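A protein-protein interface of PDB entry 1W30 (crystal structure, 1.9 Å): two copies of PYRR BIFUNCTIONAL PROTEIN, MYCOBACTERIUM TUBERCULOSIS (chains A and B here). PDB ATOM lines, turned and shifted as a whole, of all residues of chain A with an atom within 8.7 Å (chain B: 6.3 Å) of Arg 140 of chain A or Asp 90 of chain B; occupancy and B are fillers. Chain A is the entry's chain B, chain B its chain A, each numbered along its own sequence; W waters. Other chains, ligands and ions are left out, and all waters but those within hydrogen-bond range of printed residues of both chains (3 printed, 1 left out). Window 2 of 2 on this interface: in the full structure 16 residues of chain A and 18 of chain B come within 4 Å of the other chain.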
ATOM      1  N   ARG A  49       8.473  10.825  26.930  1.00  0.00           N
ATOM      2  CA  ARG A  49       7.064  10.635  26.881  1.00  0.00           C
ATOM      3  C   ARG A  49       6.700   9.273  26.318  1.00  0.00           C
ATOM      4  O   ARG A  49       7.416   8.712  25.530  1.00  0.00           O
ATOM      5  CB  ARG A  49       6.452  11.704  26.018  1.00  0.00           C
ATOM      6  CG  ARG A  49       6.798  11.647  24.545  1.00  0.00           C
ATOM      7  CD  ARG A  49       6.772  13.021  23.920  1.00  0.00           C
ATOM      8  NE  ARG A  49       6.729  12.958  22.469  1.00  0.00           N
ATOM      9  CZ  ARG A  49       7.782  12.845  21.707  1.00  0.00           C
ATOM     10  NH1 ARG A  49       9.017  12.797  22.203  1.00  0.00           N
ATOM     11  NH2 ARG A  49       7.602  12.789  20.413  1.00  0.00           N
ATOM     12  N   GLY A 109       4.531  13.474  17.403  1.00  0.00           N
ATOM     13  CA  GLY A 109       5.368  12.465  16.799  1.00  0.00           C
ATOM     14  C   GLY A 109       5.931  11.473  17.810  1.00  0.00           C
ATOM     15  O   GLY A 109       5.442  11.345  18.957  1.00  0.00           O
ATOM     16  N   ILE A 110       6.953  10.760  17.371  1.00  0.00           N
ATOM     17  CA  ILE A 110       7.583   9.756  18.239  1.00  0.00           C
ATOM     18  C   ILE A 110       9.050  10.022  18.394  1.00  0.00           C
ATOM     19  O   ILE A 110       9.783   9.197  18.969  1.00  0.00           O
ATOM     20  CB  ILE A 110       7.223   8.281  17.789  1.00  0.00           C
ATOM     21  CG1 ILE A 110       7.600   7.982  16.357  1.00  0.00           C
ATOM     22  CG2 ILE A 110       5.755   8.076  17.896  1.00  0.00           C
ATOM     23  CD1 ILE A 110       8.974   7.815  16.148  1.00  0.00           C
ATOM     24  N   ASP A 111       9.531  11.180  17.906  1.00  0.00           N
ATOM     25  CA  ASP A 111      10.986  11.416  17.991  1.00  0.00           C
ATOM     26  C   ASP A 111      11.385  11.555  19.442  1.00  0.00           C
ATOM     27  O   ASP A 111      10.769  12.293  20.160  1.00  0.00           O
ATOM     28  CB  ASP A 111      11.485  12.678  17.226  1.00  0.00           C
ATOM     29  CG  ASP A 111      11.848  12.398  15.755  1.00  0.00           C
ATOM     30  OD1 ASP A 111      11.372  11.397  15.168  1.00  0.00           O
ATOM     31  OD2 ASP A 111      12.589  13.171  15.085  1.00  0.00           O
ATOM     32  N   ASP A 112      12.412  10.822  19.854  1.00  0.00           N
ATOM     33  CA  ASP A 112      12.860  10.756  21.250  1.00  0.00           C
ATOM     34  C   ASP A 112      11.769  10.345  22.273  1.00  0.00           C
ATOM     35  O   ASP A 112      11.951  10.475  23.493  1.00  0.00           O
ATOM     36  CB  ASP A 112      13.535  12.099  21.597  1.00  0.00           C
ATOM     37  CG  ASP A 112      14.399  12.032  22.836  1.00  0.00           C
ATOM     38  OD1 ASP A 112      15.287  11.165  22.948  1.00  0.00           O
ATOM     39  OD2 ASP A 112      14.259  12.856  23.762  1.00  0.00           O
ATOM     40  N   ALA A 113      10.661   9.798  21.799  1.00  0.00           N
ATOM     41  CA  ALA A 113       9.679   9.184  22.674  1.00  0.00           C
ATOM     42  C   ALA A 113      10.069   7.748  23.083  1.00  0.00           C
ATOM     43  O   ALA A 113      11.001   7.169  22.533  1.00  0.00           O
ATOM     44  CB  ALA A 113       8.367   9.176  22.039  1.00  0.00           C
ATOM     45  N   LEU A 114       9.368   7.239  24.087  1.00  0.00           N
ATOM     46  CA  LEU A 114       9.361   5.822  24.419  1.00  0.00           C
ATOM     47  C   LEU A 114       8.135   5.276  23.743  1.00  0.00           C
ATOM     48  O   LEU A 114       7.030   5.560  24.124  1.00  0.00           O
ATOM     49  CB  LEU A 114       9.354   5.611  25.947  1.00  0.00           C
ATOM     50  CG  LEU A 114       9.399   4.141  26.456  1.00  0.00           C
ATOM     51  CD1 LEU A 114       9.350   4.079  27.976  1.00  0.00           C
ATOM     52  CD2 LEU A 114       8.226   3.396  25.997  1.00  0.00           C
ATOM     53  N   VAL A 115       8.312   4.541  22.655  1.00  0.00           N
ATOM     54  CA  VAL A 115       7.183   3.947  21.972  1.00  0.00           C
ATOM     55  C   VAL A 115       6.933   2.541  22.523  1.00  0.00           C
ATOM     56  O   VAL A 115       7.856   1.781  22.557  1.00  0.00           O
ATOM     57  CB  VAL A 115       7.482   3.829  20.453  1.00  0.00           C
ATOM     58  CG1 VAL A 115       6.453   3.008  19.800  1.00  0.00           C
ATOM     59  CG2 VAL A 115       7.560   5.273  19.817  1.00  0.00           C
ATOM     60  N   ALA A 134       8.951  -0.139  10.161  1.00  0.00           N
ATOM     61  CA  ALA A 134       7.923   0.841   9.920  1.00  0.00           C
ATOM     62  C   ALA A 134       8.070   2.067  10.849  1.00  0.00           C
ATOM     63  O   ALA A 134       7.861   3.202  10.436  1.00  0.00           O
ATOM     64  CB  ALA A 134       6.569   0.209  10.085  1.00  0.00           C
ATOM     65  N   LEU A 135       8.456   1.818  12.103  1.00  0.00           N
ATOM     66  CA  LEU A 135       8.629   2.869  13.075  1.00  0.00           C
ATOM     67  C   LEU A 135       9.759   3.791  12.656  1.00  0.00           C
ATOM     68  O   LEU A 135       9.661   5.018  12.753  1.00  0.00           O
ATOM     69  CB  LEU A 135       9.000   2.255  14.442  1.00  0.00           C
ATOM     70  CG  LEU A 135       7.978   2.492  15.534  1.00  0.00           C
ATOM     71  CD1 LEU A 135       8.572   1.955  16.866  1.00  0.00           C
ATOM     72  CD2 LEU A 135       7.631   3.890  15.672  1.00  0.00           C
ATOM     73  N   ARG A 136      10.842   3.182  12.193  1.00  0.00           N
ATOM     74  CA  ARG A 136      11.989   3.920  11.722  1.00  0.00           C
ATOM     75  C   ARG A 136      11.647   4.857  10.529  1.00  0.00           C
ATOM     76  O   ARG A 136      12.237   5.930  10.395  1.00  0.00           O
ATOM     77  CB  ARG A 136      13.127   2.961  11.401  1.00  0.00           C
ATOM     78  CG  ARG A 136      14.380   3.600  10.867  1.00  0.00           C
ATOM     79  CD  ARG A 136      15.603   2.679  10.913  1.00  0.00           C
ATOM     80  NE  ARG A 136      15.412   1.493  10.097  1.00  0.00           N
ATOM     81  CZ  ARG A 136      16.229   0.434  10.054  1.00  0.00           C
ATOM     82  NH1 ARG A 136      17.359   0.411  10.754  1.00  0.00           N
ATOM     83  NH2 ARG A 136      15.892  -0.618   9.304  1.00  0.00           N
ATOM     84  N   ASP A 137      10.698   4.464   9.703  1.00  0.00           N
ATOM     85  CA  ASP A 137      10.185   5.351   8.651  1.00  0.00           C
ATOM     86  C   ASP A 137       9.316   6.498   9.156  1.00  0.00           C
ATOM     87  O   ASP A 137       9.094   7.469   8.427  1.00  0.00           O
ATOM     88  CB  ASP A 137       9.452   4.528   7.603  1.00  0.00           C
ATOM     89  CG  ASP A 137      10.397   3.634   6.803  1.00  0.00           C
ATOM     90  OD1 ASP A 137      11.653   3.869   6.841  1.00  0.00           O
ATOM     91  OD2 ASP A 137       9.967   2.656   6.106  1.00  0.00           O
ATOM     92  N   VAL A 138       8.772   6.374  10.373  1.00  0.00           N
ATOM     93  CA  VAL A 138       7.983   7.439  11.004  1.00  0.00           C
ATOM     94  C   VAL A 138       8.904   8.409  11.721  1.00  0.00           C
ATOM     95  O   VAL A 138       8.730   9.629  11.589  1.00  0.00           O
ATOM     96  CB  VAL A 138       6.918   6.866  11.989  1.00  0.00           C
ATOM     97  CG1 VAL A 138       6.232   7.991  12.808  1.00  0.00           C
ATOM     98  CG2 VAL A 138       5.904   6.059  11.206  1.00  0.00           C
ATOM     99  N   GLY A 139       9.902   7.898  12.426  1.00  0.00           N
ATOM    100  CA  GLY A 139      10.667   8.722  13.336  1.00  0.00           C
ATOM    101  C   GLY A 139      11.782   8.006  14.061  1.00  0.00           C
ATOM    102  O   GLY A 139      12.141   6.885  13.720  1.00  0.00           O
ATOM    103  N   ARG A 140      12.349   8.656  15.068  1.00  0.00           N
ATOM    104  CA  ARG A 140      13.497   8.119  15.772  1.00  0.00           C
ATOM    105  C   ARG A 140      13.182   8.115  17.264  1.00  0.00           C
ATOM    106  O   ARG A 140      13.469   9.045  17.970  1.00  0.00           O
ATOM    107  CB  ARG A 140      14.776   8.919  15.488  1.00  0.00           C
ATOM    108  CG  ARG A 140      16.042   8.083  15.468  1.00  0.00           C
ATOM    109  CD  ARG A 140      16.222   7.030  16.610  1.00  0.00           C
ATOM    110  NE  ARG A 140      17.598   6.475  16.682  1.00  0.00           N
ATOM    111  CZ  ARG A 140      18.329   6.341  17.804  1.00  0.00           C
ATOM    112  NH1 ARG A 140      17.855   6.736  18.982  1.00  0.00           N
ATOM    113  NH2 ARG A 140      19.553   5.821  17.751  1.00  0.00           N
ATOM    114  N   PRO A 141      12.569   7.053  17.743  1.00  0.00           N
ATOM    115  CA  PRO A 141      12.295   6.959  19.170  1.00  0.00           C
ATOM    116  C   PRO A 141      13.538   6.829  20.023  1.00  0.00           C
ATOM    117  O   PRO A 141      14.574   6.373  19.629  1.00  0.00           O
ATOM    118  CB  PRO A 141      11.350   5.754  19.279  1.00  0.00           C
ATOM    119  CG  PRO A 141      11.322   5.112  17.971  1.00  0.00           C
ATOM    120  CD  PRO A 141      12.037   5.925  16.961  1.00  0.00           C
ATOM    121  N   ARG A 142      13.455   7.287  21.260  1.00  0.00           N
ATOM    122  CA  ARG A 142      14.547   7.050  22.160  1.00  0.00           C
ATOM    123  C   ARG A 142      14.619   5.540  22.515  1.00  0.00           C
ATOM    124  O   ARG A 142      15.713   4.977  22.679  1.00  0.00           O
ATOM    125  CB  ARG A 142      14.333   7.813  23.443  1.00  0.00           C
ATOM    126  CG  ARG A 142      15.589   7.767  24.251  1.00  0.00           C
ATOM    127  CD  ARG A 142      15.423   8.367  25.621  1.00  0.00           C
ATOM    128  NE  ARG A 142      15.122   9.797  25.516  1.00  0.00           N
ATOM    129  CZ  ARG A 142      14.933  10.579  26.566  1.00  0.00           C
ATOM    130  NH1 ARG A 142      14.952  10.074  27.787  1.00  0.00           N
ATOM    131  NH2 ARG A 142      14.711  11.862  26.396  1.00  0.00           N
ATOM    132  N   ALA A 143      13.451   4.935  22.647  1.00  0.00           N
ATOM    133  CA  ALA A 143      13.353   3.529  23.021  1.00  0.00           C
ATOM    134  C   ALA A 143      12.005   2.906  22.526  1.00  0.00           C
ATOM    135  O   ALA A 143      11.002   3.580  22.271  1.00  0.00           O
ATOM    136  CB  ALA A 143      13.555   3.363  24.534  1.00  0.00           C
ATOM    137  N   VAL A 144      12.028   1.582  22.366  1.00  0.00           N
ATOM    138  CA  VAL A 144      10.901   0.846  21.895  1.00  0.00           C
ATOM    139  C   VAL A 144      10.770  -0.386  22.782  1.00  0.00           C
ATOM    140  O   VAL A 144      11.719  -1.100  22.974  1.00  0.00           O
ATOM    141  CB  VAL A 144      11.054   0.354  20.452  1.00  0.00           C
ATOM    142  CG1 VAL A 144       9.735  -0.190  19.983  1.00  0.00           C
ATOM    143  CG2 VAL A 144      11.486   1.518  19.532  1.00  0.00           C
ATOM    144  N   TYR B  88      25.101   0.029   8.614  1.00  0.00           N
ATOM    145  CA  TYR B  88      23.766  -0.171   9.190  1.00  0.00           C
ATOM    146  C   TYR B  88      23.558   0.531  10.523  1.00  0.00           C
ATOM    147  O   TYR B  88      22.525   0.366  11.157  1.00  0.00           O
ATOM    148  CB  TYR B  88      23.518  -1.653   9.350  1.00  0.00           C
ATOM    149  CG  TYR B  88      23.644  -2.347   8.066  1.00  0.00           C
ATOM    150  CD1 TYR B  88      24.888  -2.782   7.608  1.00  0.00           C
ATOM    151  CD2 TYR B  88      22.539  -2.534   7.241  1.00  0.00           C
ATOM    152  CE1 TYR B  88      25.015  -3.442   6.411  1.00  0.00           C
ATOM    153  CE2 TYR B  88      22.668  -3.192   6.012  1.00  0.00           C
ATOM    154  CZ  TYR B  88      23.902  -3.619   5.612  1.00  0.00           C
ATOM    155  OH  TYR B  88      24.065  -4.274   4.452  1.00  0.00           O
ATOM    156  N   ARG B  89      24.545   1.324  10.929  1.00  0.00           N
ATOM    157  CA  ARG B  89      24.514   2.025  12.191  1.00  0.00           C
ATOM    158  C   ARG B  89      23.637   3.228  12.015  1.00  0.00           C
ATOM    159  O   ARG B  89      23.527   3.739  10.904  1.00  0.00           O
ATOM    160  CB  ARG B  89      25.923   2.480  12.588  1.00  0.00           C
ATOM    161  CG  ARG B  89      26.432   1.848  13.864  1.00  0.00           C
ATOM    162  CD  ARG B  89      27.916   2.040  14.093  1.00  0.00           C
ATOM    163  NE  ARG B  89      28.437   1.028  15.019  1.00  0.00           N
ATOM    164  CZ  ARG B  89      29.438   0.177  14.759  1.00  0.00           C
ATOM    165  NH1 ARG B  89      30.087   0.191  13.590  1.00  0.00           N
ATOM    166  NH2 ARG B  89      29.798  -0.696  15.699  1.00  0.00           N
ATOM    167  N   ASP B  90      23.047   3.696  13.119  1.00  0.00           N
ATOM    168  CA  ASP B  90      22.061   4.799  13.115  1.00  0.00           C
ATOM    169  C   ASP B  90      22.754   6.081  12.668  1.00  0.00           C
ATOM    170  O   ASP B  90      23.820   6.408  13.184  1.00  0.00           O
ATOM    171  CB  ASP B  90      21.422   5.041  14.520  1.00  0.00           C
ATOM    172  CG  ASP B  90      21.170   3.744  15.325  1.00  0.00           C
ATOM    173  OD1 ASP B  90      22.123   2.951  15.548  1.00  0.00           O
ATOM    174  OD2 ASP B  90      20.042   3.445  15.789  1.00  0.00           O
ATOM    175  N   ARG B 126      20.969  -1.733  20.001  1.00  0.00           N
ATOM    176  CA  ARG B 126      20.981  -1.075  18.673  1.00  0.00           C
ATOM    177  C   ARG B 126      21.958  -1.727  17.732  1.00  0.00           C
ATOM    178  O   ARG B 126      21.693  -1.820  16.496  1.00  0.00           O
ATOM    179  CB  ARG B 126      21.239   0.430  18.790  1.00  0.00           C
ATOM    180  CG  ARG B 126      19.944   1.196  19.080  1.00  0.00           C
ATOM    181  CD  ARG B 126      20.144   2.612  19.481  1.00  0.00           C
ATOM    182  NE  ARG B 126      18.956   3.249  20.058  1.00  0.00           N
ATOM    183  CZ  ARG B 126      17.741   3.381  19.518  1.00  0.00           C
ATOM    184  NH1 ARG B 126      17.403   2.922  18.319  1.00  0.00           N
ATOM    185  NH2 ARG B 126      16.828   4.017  20.238  1.00  0.00           N
ATOM    186  N   SER B 127      23.092  -2.205  18.277  1.00  0.00           N
ATOM    187  CA  SER B 127      24.063  -2.951  17.511  1.00  0.00           C
ATOM    188  C   SER B 127      23.481  -4.248  16.954  1.00  0.00           C
ATOM    189  O   SER B 127      23.751  -4.631  15.815  1.00  0.00           O
ATOM    190  CB  SER B 127      25.258  -3.290  18.355  1.00  0.00           C
ATOM    191  OG  SER B 127      26.073  -2.166  18.489  1.00  0.00           O
ATOM    192  N   ARG B 129      20.229  -4.768  16.361  1.00  0.00           N
ATOM    193  CA  ARG B 129      19.258  -4.375  15.347  1.00  0.00           C
ATOM    194  C   ARG B 129      20.013  -4.070  14.057  1.00  0.00           C
ATOM    195  O   ARG B 129      19.659  -4.523  12.977  1.00  0.00           O
ATOM    196  CB  ARG B 129      18.462  -3.152  15.797  1.00  0.00           C
ATOM    197  CG  ARG B 129      17.219  -2.935  14.937  1.00  0.00           C
ATOM    198  CD  ARG B 129      17.493  -2.115  13.690  1.00  0.00           C
ATOM    199  NE  ARG B 129      16.275  -1.970  12.892  1.00  0.00           N
ATOM    200  CZ  ARG B 129      15.321  -1.084  13.167  1.00  0.00           C
ATOM    201  NH1 ARG B 129      15.441  -0.252  14.197  1.00  0.00           N
ATOM    202  NH2 ARG B 129      14.246  -1.012  12.401  1.00  0.00           N
ATOM    203  N   SER B 130      21.090  -3.335  14.170  1.00  0.00           N
ATOM    204  CA  SER B 130      21.915  -3.127  12.978  1.00  0.00           C
ATOM    205  C   SER B 130      22.378  -4.426  12.315  1.00  0.00           C
ATOM    206  O   SER B 130      22.420  -4.513  11.106  1.00  0.00           O
ATOM    207  CB  SER B 130      23.106  -2.294  13.321  1.00  0.00           C
ATOM    208  OG  SER B 130      22.667  -1.007  13.646  1.00  0.00           O
ATOM    209  N   GLU B 156      17.075  -0.413  24.650  1.00  0.00           N
ATOM    210  CA  GLU B 156      16.266   0.564  23.948  1.00  0.00           C
ATOM    211  C   GLU B 156      15.368  -0.059  22.884  1.00  0.00           C
ATOM    212  O   GLU B 156      14.544   0.616  22.269  1.00  0.00           O
ATOM    213  CB  GLU B 156      17.189   1.611  23.334  1.00  0.00           C
ATOM    214  CG  GLU B 156      17.951   2.361  24.419  1.00  0.00           C
ATOM    215  CD  GLU B 156      18.912   3.413  23.884  1.00  0.00           C
ATOM    216  OE1 GLU B 156      19.007   3.613  22.645  1.00  0.00           O
ATOM    217  OE2 GLU B 156      19.635   3.966  24.742  1.00  0.00           O
HETATM  218  O   HOH W   1      19.981  -0.463  11.941  1.00  0.00           O
HETATM  219  O   HOH W   2      18.184   2.543  13.232  1.00  0.00           O
HETATM  220  O   HOH W   3      20.135  -0.483   8.936  1.00  0.00           O
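No position is printed for both chains.
Of the 19 printed residues of chain A, 6 touch a printed residue of chain B. Among the printed residues, 8 pairs touch across the chains.
Water W1 lies within hydrogen-bond range of the backbone carbonyl oxygen (O) of Tyr 88 of chain B (2.8 Å), the guanidinium group (NH1) of Arg 136 of chain A (3.0 Å) and the side-chain hydroxyl (OG) of Ser 130 of chain B (3.2 Å). Water W2 bridges OD2 of Asp 90 of chain B (3.3 Å) and NH1 of Arg 136 of chain A (3.4 Å). Water W3 bridges the backbone carbonyl oxygen of Tyr 88 of chain B (3.4 Å) and the guanidinium group of Arg 136 of chain A (3.4 Å).
The side-chain carboxylate (OD2) of Asp 90 of chain B is in salt-bridge range of the guanidinium group (NH1) of Arg 126 of chain B (3.7 Å). The side-chain hydroxyl (OG) of Ser 130 of chain B is in hydrogen-bond range of the backbone carbonyl oxygen (O) of Arg 126 of chain B, at 3.1 Å. The side-chain carboxylate (OD2) of Asp 112 of chain A lies within salt-bridge range of the guanidinium group (NH2) of Arg 142 of chain A (2.9 Å). The backbone carbonyl oxygen (O) of Ala 113 of chain A lies within hydrogen-bond range of the backbone NH (N) of Arg 142 of chain A, at 2.8 Å. N of Ala 143 of chain A lies within hydrogen-bond range of O of Ala 113 of chain A, at 3.3 Å. The backbone carbonyl oxygen (O) of Ala 143 of chain A lies within hydrogen-bond range of the backbone NH (N) of Val 115 of chain A.
NH2 of Arg 140 of chain A is in salt-bridge range of OD2 of Asp 90 of chain B (3.1 Å). NH2 of Arg 126 of chain B lies within hydrogen-bond range of O of Pro 141 of chain A (3.3 Å). The guanidinium group (NH2) of Arg 126 of chain B sits at hydrogen-bond distance from the backbone carbonyl oxygen (O) of Arg 142 of chain A, at 2.9 Å. The backbone carbonyl oxygen (O) of Glu 156 of chain B lies within hydrogen-bond range of the backbone NH (N) of Val 144 of chain A (2.7 Å). The guanidinium group (NE) of Arg 129 of chain B sits close to the guanidinium group (NH1) of Arg 136 of chain A. The guanidinium group (NH1) of Arg 140 of chain A lies close to the guanidinium group (NH2) of Arg 126 of chain B.
Asp 111 of chain A touches none of the printed residues of chain B. Of the printed residues of chain B, Arg 136 of chain A touches Arg 129 (3.4 Å). Arg 140 of chain A touches just these residues of chain B: Asp 90 (3.1 Å) and Arg 126 (3.2 Å). Of the printed residues of chain A, Asp 90 of chain B touches Arg 140. Printed residues of chain A within 4 Å of Glu 156 of chain B: Arg 142, Ala 143 and Val 144.
Among the printed residues, pairs that only touch across the chains: Ala 143 of chain A with Glu 156 of chain B and Arg 142 of chain A with Glu 156 of chain B.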
